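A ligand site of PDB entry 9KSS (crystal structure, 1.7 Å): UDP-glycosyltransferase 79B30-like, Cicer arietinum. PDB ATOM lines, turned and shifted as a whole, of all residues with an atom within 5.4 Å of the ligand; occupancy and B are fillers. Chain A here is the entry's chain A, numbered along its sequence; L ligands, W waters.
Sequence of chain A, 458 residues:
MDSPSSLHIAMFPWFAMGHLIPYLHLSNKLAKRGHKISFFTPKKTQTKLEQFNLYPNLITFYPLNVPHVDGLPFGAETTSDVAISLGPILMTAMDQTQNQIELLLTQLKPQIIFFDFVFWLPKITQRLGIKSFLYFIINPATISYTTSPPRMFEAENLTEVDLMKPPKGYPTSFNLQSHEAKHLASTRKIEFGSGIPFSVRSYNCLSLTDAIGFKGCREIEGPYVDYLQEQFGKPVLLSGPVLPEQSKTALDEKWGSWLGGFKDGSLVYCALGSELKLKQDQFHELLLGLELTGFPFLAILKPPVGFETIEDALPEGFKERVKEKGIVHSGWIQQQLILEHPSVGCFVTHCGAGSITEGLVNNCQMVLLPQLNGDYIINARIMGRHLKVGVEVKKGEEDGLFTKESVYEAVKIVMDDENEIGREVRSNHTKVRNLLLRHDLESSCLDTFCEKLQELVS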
ATOM      1  N   MET A  17      -1.196 -21.683 -21.081  1.00  0.00           N
ATOM      2  CA  MET A  17      -1.549 -20.577 -20.197  1.00  0.00           C
ATOM      3  C   MET A  17      -2.753 -20.920 -19.337  1.00  0.00           C
ATOM      4  O   MET A  17      -2.821 -20.513 -18.166  1.00  0.00           O
ATOM      5  CB  MET A  17      -1.807 -19.316 -21.009  1.00  0.00           C
ATOM      6  CG  MET A  17      -0.577 -18.707 -21.721  1.00  0.00           C
ATOM      7  SD  MET A  17       0.915 -18.549 -20.712  1.00  0.00           S
ATOM      8  CE  MET A  17       0.434 -17.197 -19.628  1.00  0.00           C
ATOM      9  N   GLY A  18      -3.684 -21.688 -19.884  1.00  0.00           N
ATOM     10  CA  GLY A  18      -4.880 -22.071 -19.120  1.00  0.00           C
ATOM     11  C   GLY A  18      -4.622 -23.071 -18.020  1.00  0.00           C
ATOM     12  O   GLY A  18      -5.532 -23.345 -17.223  1.00  0.00           O
ATOM     13  N   ILE A  21      -1.822 -20.451 -15.378  1.00  0.00           N
ATOM     14  CA  ILE A  21      -2.469 -19.357 -14.650  1.00  0.00           C
ATOM     15  C   ILE A  21      -3.258 -19.887 -13.446  1.00  0.00           C
ATOM     16  O   ILE A  21      -3.033 -19.383 -12.333  1.00  0.00           O
ATOM     17  CB  ILE A  21      -3.344 -18.519 -15.604  1.00  0.00           C
ATOM     18  CG1 ILE A  21      -2.459 -17.644 -16.483  1.00  0.00           C
ATOM     19  CG2 ILE A  21      -4.252 -17.631 -14.819  1.00  0.00           C
ATOM     20  CD1 ILE A  21      -3.223 -16.918 -17.582  1.00  0.00           C
ATOM     21  N   LEU A 272     -11.929 -16.164 -27.359  1.00  0.00           N
ATOM     22  CA  LEU A 272     -11.929 -17.613 -27.467  1.00  0.00           C
ATOM     23  C   LEU A 272     -10.619 -18.197 -26.951  1.00  0.00           C
ATOM     24  O   LEU A 272     -10.090 -19.178 -27.503  1.00  0.00           O
ATOM     25  CB  LEU A 272     -12.211 -18.053 -28.899  1.00  0.00           C
ATOM     26  CG  LEU A 272     -13.435 -17.393 -29.557  1.00  0.00           C
ATOM     27  CD1 LEU A 272     -13.553 -17.881 -30.993  1.00  0.00           C
ATOM     28  CD2 LEU A 272     -14.758 -17.660 -28.778  1.00  0.00           C
ATOM     29  N   GLY A 273     -10.054 -17.587 -25.911  1.00  0.00           N
ATOM     30  CA  GLY A 273      -8.882 -18.117 -25.246  1.00  0.00           C
ATOM     31  C   GLY A 273      -7.596 -17.804 -26.002  1.00  0.00           C
ATOM     32  O   GLY A 273      -7.548 -16.973 -26.907  1.00  0.00           O
ATOM     33  N   SER A 274      -6.547 -18.524 -25.605  1.00  0.00           N
ATOM     34  CA  SER A 274      -5.197 -18.223 -26.043  1.00  0.00           C
ATOM     35  C   SER A 274      -4.624 -19.257 -26.998  1.00  0.00           C
ATOM     36  O   SER A 274      -3.460 -19.134 -27.384  1.00  0.00           O
ATOM     37  CB  SER A 274      -4.253 -18.119 -24.831  1.00  0.00           C
ATOM     38  OG  SER A 274      -4.199 -19.380 -24.175  1.00  0.00           O
ATOM     39  N   GLU A 275      -5.394 -20.290 -27.354  1.00  0.00           N
ATOM     40  CA  GLU A 275      -4.864 -21.411 -28.111  1.00  0.00           C
ATOM     41  C   GLU A 275      -5.388 -21.479 -29.533  1.00  0.00           C
ATOM     42  O   GLU A 275      -4.618 -21.760 -30.457  1.00  0.00           O
ATOM     43  CB  GLU A 275      -5.182 -22.735 -27.412  1.00  0.00           C
ATOM     44  CG  GLU A 275      -4.556 -22.914 -26.068  1.00  0.00           C
ATOM     45  CD  GLU A 275      -4.923 -24.249 -25.418  1.00  0.00           C
ATOM     46  OE1 GLU A 275      -4.000 -25.033 -25.153  1.00  0.00           O
ATOM     47  OE2 GLU A 275      -6.129 -24.553 -25.237  1.00  0.00           O
ATOM     48  N   ILE A 300     -11.454 -10.500 -29.081  1.00  0.00           N
ATOM     49  CA  ILE A 300     -10.053 -10.904 -28.911  1.00  0.00           C
ATOM     50  C   ILE A 300      -9.895 -12.246 -29.625  1.00  0.00           C
ATOM     51  O   ILE A 300     -10.320 -13.285 -29.119  1.00  0.00           O
ATOM     52  CB  ILE A 300      -9.669 -10.994 -27.434  1.00  0.00           C
ATOM     53  CG1 ILE A 300     -10.012  -9.681 -26.727  1.00  0.00           C
ATOM     54  CG2 ILE A 300      -8.169 -11.374 -27.290  1.00  0.00           C
ATOM     55  CD1 ILE A 300      -9.243  -8.478 -27.313  1.00  0.00           C
ATOM     56  N   GLY A 331      -3.811  -9.374 -29.888  1.00  0.00           N
ATOM     57  CA  GLY A 331      -2.823  -9.555 -28.844  1.00  0.00           C
ATOM     58  C   GLY A 331      -3.403 -10.035 -27.525  1.00  0.00           C
ATOM     59  O   GLY A 331      -4.613  -9.973 -27.298  1.00  0.00           O
ATOM     60  N   TRP A 332      -2.512 -10.538 -26.660  1.00  0.00           N
ATOM     61  CA  TRP A 332      -2.866 -10.897 -25.288  1.00  0.00           C
ATOM     62  C   TRP A 332      -3.332  -9.675 -24.505  1.00  0.00           C
ATOM     63  O   TRP A 332      -2.669  -8.630 -24.524  1.00  0.00           O
ATOM     64  CB  TRP A 332      -1.643 -11.519 -24.605  1.00  0.00           C
ATOM     65  CG  TRP A 332      -1.844 -11.902 -23.169  1.00  0.00           C
ATOM     66  CD1 TRP A 332      -1.714 -11.095 -22.078  1.00  0.00           C
ATOM     67  CD2 TRP A 332      -2.219 -13.192 -22.671  1.00  0.00           C
ATOM     68  NE1 TRP A 332      -1.986 -11.811 -20.921  1.00  0.00           N
ATOM     69  CE2 TRP A 332      -2.311 -13.094 -21.278  1.00  0.00           C
ATOM     70  CE3 TRP A 332      -2.512 -14.418 -23.292  1.00  0.00           C
ATOM     71  CZ2 TRP A 332      -2.669 -14.178 -20.473  1.00  0.00           C
ATOM     72  CZ3 TRP A 332      -2.868 -15.485 -22.500  1.00  0.00           C
ATOM     73  CH2 TRP A 332      -2.935 -15.374 -21.103  1.00  0.00           C
ATOM     74  N   ILE A 333      -4.466  -9.785 -23.818  1.00  0.00           N
ATOM     75  CA  ILE A 333      -4.940  -8.669 -23.003  1.00  0.00           C
ATOM     76  C   ILE A 333      -5.230  -9.180 -21.601  1.00  0.00           C
ATOM     77  O   ILE A 333      -5.205 -10.385 -21.339  1.00  0.00           O
ATOM     78  CB  ILE A 333      -6.175  -7.975 -23.614  1.00  0.00           C
ATOM     79  CG1 ILE A 333      -7.127  -8.973 -24.272  1.00  0.00           C
ATOM     80  CG2 ILE A 333      -5.740  -6.922 -24.636  1.00  0.00           C
ATOM     81  CD1 ILE A 333      -7.800  -9.923 -23.332  1.00  0.00           C
ATOM     82  N   GLN A 334      -5.496  -8.241 -20.686  1.00  0.00           N
ATOM     83  CA  GLN A 334      -5.784  -8.576 -19.297  1.00  0.00           C
ATOM     84  C   GLN A 334      -7.268  -8.910 -19.186  1.00  0.00           C
ATOM     85  O   GLN A 334      -8.086  -8.108 -18.745  1.00  0.00           O
ATOM     86  CB  GLN A 334      -5.417  -7.427 -18.369  1.00  0.00           C
ATOM     87  CG  GLN A 334      -3.963  -7.007 -18.479  1.00  0.00           C
ATOM     88  CD  GLN A 334      -3.735  -5.617 -17.951  1.00  0.00           C
ATOM     89  OE1 GLN A 334      -3.954  -4.644 -18.656  1.00  0.00           O
ATOM     90  NE2 GLN A 334      -3.296  -5.521 -16.698  1.00  0.00           N
ATOM     91  N   GLN A 335      -7.610 -10.137 -19.606  1.00  0.00           N
ATOM     92  CA  GLN A 335      -9.017 -10.530 -19.717  1.00  0.00           C
ATOM     93  C   GLN A 335      -9.743 -10.402 -18.385  1.00  0.00           C
ATOM     94  O   GLN A 335     -10.906  -9.956 -18.327  1.00  0.00           O
ATOM     95  CB  GLN A 335      -9.142 -11.969 -20.231  1.00  0.00           C
ATOM     96  CG  GLN A 335     -10.565 -12.499 -20.081  1.00  0.00           C
ATOM     97  CD  GLN A 335     -10.835 -13.750 -20.870  1.00  0.00           C
ATOM     98  OE1 GLN A 335     -10.829 -13.724 -22.111  1.00  0.00           O
ATOM     99  NE2 GLN A 335     -11.110 -14.859 -20.166  1.00  0.00           N
ATOM    100  N   GLN A 336      -9.091 -10.827 -17.299  1.00  0.00           N
ATOM    101  CA  GLN A 336      -9.740 -10.777 -15.986  1.00  0.00           C
ATOM    102  C   GLN A 336     -10.127  -9.351 -15.629  1.00  0.00           C
ATOM    103  O   GLN A 336     -11.216  -9.118 -15.078  1.00  0.00           O
ATOM    104  CB  GLN A 336      -8.815 -11.391 -14.932  1.00  0.00           C
ATOM    105  CG  GLN A 336      -9.274 -11.266 -13.472  1.00  0.00           C
ATOM    106  CD  GLN A 336      -8.119 -11.446 -12.499  1.00  0.00           C
ATOM    107  OE1 GLN A 336      -7.245 -12.309 -12.703  1.00  0.00           O
ATOM    108  NE2 GLN A 336      -8.087 -10.633 -11.459  1.00  0.00           N
ATOM    109  N   HIS A 350     -15.608 -19.086 -25.447  1.00  0.00           N
ATOM    110  CA  HIS A 350     -15.389 -20.429 -25.948  1.00  0.00           C
ATOM    111  C   HIS A 350     -15.526 -21.487 -24.866  1.00  0.00           C
ATOM    112  O   HIS A 350     -15.350 -22.678 -25.177  1.00  0.00           O
ATOM    113  CB  HIS A 350     -13.991 -20.552 -26.588  1.00  0.00           C
ATOM    114  CG  HIS A 350     -12.850 -20.660 -25.608  1.00  0.00           C
ATOM    115  ND1 HIS A 350     -12.673 -19.805 -24.550  1.00  0.00           N
ATOM    116  CD2 HIS A 350     -11.793 -21.519 -25.568  1.00  0.00           C
ATOM    117  CE1 HIS A 350     -11.574 -20.132 -23.883  1.00  0.00           C
ATOM    118  NE2 HIS A 350     -11.023 -21.168 -24.485  1.00  0.00           N
ATOM    119  N   GLY A 352     -13.752 -22.211 -22.224  1.00  0.00           N
ATOM    120  CA  GLY A 352     -12.604 -22.676 -21.448  1.00  0.00           C
ATOM    121  C   GLY A 352     -12.854 -22.499 -19.957  1.00  0.00           C
ATOM    122  O   GLY A 352     -13.529 -21.562 -19.528  1.00  0.00           O
ATOM    123  N   ALA A 353     -12.355 -23.440 -19.157  1.00  0.00           N
ATOM    124  CA  ALA A 353     -12.750 -23.466 -17.750  1.00  0.00           C
ATOM    125  C   ALA A 353     -12.251 -22.234 -17.006  1.00  0.00           C
ATOM    126  O   ALA A 353     -12.896 -21.781 -16.058  1.00  0.00           O
ATOM    127  CB  ALA A 353     -12.250 -24.735 -17.079  1.00  0.00           C
ATOM    128  N   GLY A 354     -11.137 -21.644 -17.455  1.00  0.00           N
ATOM    129  CA  GLY A 354     -10.657 -20.440 -16.789  1.00  0.00           C
ATOM    130  C   GLY A 354     -11.527 -19.251 -17.106  1.00  0.00           C
ATOM    131  O   GLY A 354     -11.875 -18.456 -16.216  1.00  0.00           O
ATOM    132  N   SER A 355     -11.907 -19.120 -18.386  1.00  0.00           N
ATOM    133  CA  SER A 355     -12.768 -18.020 -18.803  1.00  0.00           C
ATOM    134  C   SER A 355     -14.152 -18.140 -18.173  1.00  0.00           C
ATOM    135  O   SER A 355     -14.754 -17.124 -17.828  1.00  0.00           O
ATOM    136  CB  SER A 355     -12.881 -18.016 -20.321  1.00  0.00           C
ATOM    137  OG  SER A 355     -11.642 -17.662 -20.909  1.00  0.00           O
ATOM    138  N   ILE A 356     -14.650 -19.365 -18.030  1.00  0.00           N
ATOM    139  CA  ILE A 356     -15.951 -19.566 -17.366  1.00  0.00           C
ATOM    140  C   ILE A 356     -15.908 -19.040 -15.936  1.00  0.00           C
ATOM    141  O   ILE A 356     -16.835 -18.346 -15.480  1.00  0.00           O
ATOM    142  CB  ILE A 356     -16.351 -21.056 -17.393  1.00  0.00           C
ATOM    143  CG1 ILE A 356     -16.756 -21.494 -18.820  1.00  0.00           C
ATOM    144  CG2 ILE A 356     -17.491 -21.342 -16.392  1.00  0.00           C
ATOM    145  CD1 ILE A 356     -17.932 -20.746 -19.420  1.00  0.00           C
ATOM    146  N   GLU A 358     -13.993 -16.786 -14.687  1.00  0.00           N
ATOM    147  CA  GLU A 358     -13.849 -15.343 -14.713  1.00  0.00           C
ATOM    148  C   GLU A 358     -15.162 -14.673 -15.077  1.00  0.00           C
ATOM    149  O   GLU A 358     -15.511 -13.619 -14.521  1.00  0.00           O
ATOM    150  CB  GLU A 358     -12.758 -14.988 -15.730  1.00  0.00           C
ATOM    151  CG  GLU A 358     -11.331 -15.029 -15.133  1.00  0.00           C
ATOM    152  CD  GLU A 358     -10.250 -15.383 -16.169  1.00  0.00           C
ATOM    153  OE1 GLU A 358     -10.363 -14.936 -17.336  1.00  0.00           O
ATOM    154  OE2 GLU A 358      -9.237 -16.027 -15.785  1.00  0.00           O
ATOM    155  N   TYR A 376     -14.651 -27.813 -23.414  1.00  0.00           N
ATOM    156  CA  TYR A 376     -15.465 -26.652 -23.778  1.00  0.00           C
ATOM    157  C   TYR A 376     -16.910 -27.049 -23.977  1.00  0.00           C
ATOM    158  O   TYR A 376     -17.840 -26.347 -23.526  1.00  0.00           O
ATOM    159  CB  TYR A 376     -14.946 -25.992 -25.057  1.00  0.00           C
ATOM    160  CG  TYR A 376     -13.478 -25.606 -25.065  1.00  0.00           C
ATOM    161  CD1 TYR A 376     -12.748 -25.469 -23.880  1.00  0.00           C
ATOM    162  CD2 TYR A 376     -12.814 -25.396 -26.273  1.00  0.00           C
ATOM    163  CE1 TYR A 376     -11.370 -25.120 -23.910  1.00  0.00           C
ATOM    164  CE2 TYR A 376     -11.482 -25.081 -26.308  1.00  0.00           C
ATOM    165  CZ  TYR A 376     -10.764 -24.936 -25.124  1.00  0.00           C
ATOM    166  OH  TYR A 376      -9.422 -24.616 -25.181  1.00  0.00           O
HETATM  167  N1  LIG L   1      -6.317 -14.912 -21.026  1.00  0.00           N
HETATM  168  C1  LIG L   1      -5.864 -13.608 -20.870  1.00  0.00           C
HETATM  169  N2  LIG L   1      -5.703 -12.921 -22.045  1.00  0.00           N
HETATM  170  C2  LIG L   1      -5.910 -13.393 -23.328  1.00  0.00           C
HETATM  171  C3  LIG L   1      -6.360 -14.749 -23.405  1.00  0.00           C
HETATM  172  C4  LIG L   1      -6.539 -15.450 -22.264  1.00  0.00           C
HETATM  173  O1  LIG L   1      -5.650 -13.106 -19.776  1.00  0.00           O
HETATM  174  O2  LIG L   1      -5.733 -12.635 -24.280  1.00  0.00           O
HETATM  175  C5  LIG L   1      -6.436 -15.733 -19.796  1.00  0.00           C
HETATM  176  C6  LIG L   1      -7.871 -15.956 -19.334  1.00  0.00           C
HETATM  177  O3  LIG L   1      -8.225 -14.877 -18.495  1.00  0.00           O
HETATM  178  C7  LIG L   1      -7.733 -17.299 -18.602  1.00  0.00           C
HETATM  179  C8  LIG L   1      -6.695 -18.032 -19.462  1.00  0.00           C
HETATM  180  O4  LIG L   1      -5.881 -16.998 -20.076  1.00  0.00           O
HETATM  181  O5  LIG L   1      -7.278 -17.125 -17.268  1.00  0.00           O
HETATM  182  C9  LIG L   1      -7.272 -18.872 -20.576  1.00  0.00           C
HETATM  183  O6  LIG L   1      -7.780 -20.071 -19.974  1.00  0.00           O
HETATM  184  P1  LIG L   1      -9.083 -20.778 -20.560  1.00  0.00           P
HETATM  185  O7  LIG L   1     -10.263 -19.865 -20.526  1.00  0.00           O
HETATM  186  O8  LIG L   1      -9.197 -22.124 -19.891  1.00  0.00           O
HETATM  187  O9  LIG L   1      -8.762 -20.893 -22.120  1.00  0.00           O
HETATM  188  P2  LIG L   1      -7.571 -21.380 -23.082  1.00  0.00           P
HETATM  189  O10 LIG L   1      -8.291 -22.049 -24.244  1.00  0.00           O
HETATM  190  O11 LIG L   1      -6.836 -20.117 -23.494  1.00  0.00           O
HETATM  191  O12 LIG L   1      -6.697 -22.362 -22.316  1.00  0.00           O
HETATM  192  O   HOH W   1      -5.592 -24.958 -22.132  1.00  0.00           O
HETATM  193  O   HOH W   2      -4.133 -22.551 -22.562  1.00  0.00           O
HETATM  194  O   HOH W   3      -7.951 -22.370 -17.260  1.00  0.00           O
HETATM  195  O   HOH W   4      -7.350 -19.590 -16.006  1.00  0.00           O
HETATM  196  O   HOH W   5      -8.170 -21.124 -26.855  1.00  0.00           O
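O3 of the ligand lies within hydrogen-bond range of OE1 of Glu 358.
The backbone NH (N) of Ser 355 is in hydrogen-bond range of an oxygen (O7) of the ligand (2.8 Å).
OG of Ser 355 sits at hydrogen-bond distance from O7 of the ligand (2.6 Å).
N of Ser 274 sits at hydrogen-bond distance from O11 of the ligand (2.7 Å).
The side-chain hydroxyl (OG) of Ser 274 is in hydrogen-bond range of an oxygen (O11) of the ligand.
The backbone NH (N) of Ile 333 lies within hydrogen-bond range of an oxygen (O2) of the ligand (3.2 Å).
N2 of the ligand is in hydrogen-bond range of O of Ile 333 (2.7 Å).
NE2 of His 350 sits at hydrogen-bond distance from O10 of the ligand.
The side-chain hydroxyl (OH) of Tyr 376 is in hydrogen-bond range of an oxygen (O10) of the ligand.
An oxygen (O8) of the ligand lies within hydrogen-bond range of the backbone NH (N) of Gly 354, 3.2 Å away.
The side-chain amide nitrogen (NE2) of Gln 335 sits at hydrogen-bond distance from an oxygen (O3) of the ligand (3.3 Å).
An oxygen (O8) of the ligand is in hydrogen-bond range of the backbone NH (N) of Ala 353, at 3.5 Å.
NE2 of Gln 335 is in hydrogen-bond range of OE1 of Glu 358 (2.9 Å).
OG of Ser 355 is in hydrogen-bond range of NE2 of Gln 335, at 2.9 Å.
The side-chain carboxylate of Glu 275 lies within hydrogen-bond range of the side-chain hydroxyl of Tyr 376, at 3.3 Å.
An oxygen (O10) of the ligand sits close to the side-chain carboxylate of Glu 275 (3.5 Å).
Gly 18 touches the ligand.
Ile 21 touches the ligand.
Gly 273 touches the ligand.
Trp 332 touches the ligand.
Gly 352 touches the ligand.
Hydrophobic or aromatic side chains within 4 Å of the ligand: Ile 21, Trp 332, Ile 333, His 350 and Tyr 376.
Water W2 lies within hydrogen-bond range of O12 of the ligand, N of Gly 18 and N of Met 17.
Water W5 lies within hydrogen-bond range of O10 of the ligand (2.8 Å), O of Leu 272 (2.8 Å), N of Glu 275 (2.9 Å) and N of Ser 274 (3.3 Å).
Water W1 bridges an oxygen (O12) of the ligand (2.8 Å) and the side-chain carboxylate (OE2) of Glu 275 (3.2 Å).
Water W3 lies within hydrogen-bond range of the backbone carbonyl oxygen of Gly 18 (2.6 Å), an oxygen (O8) of the ligand (2.9 Å) and the backbone NH of Gly 354 (3.3 Å).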
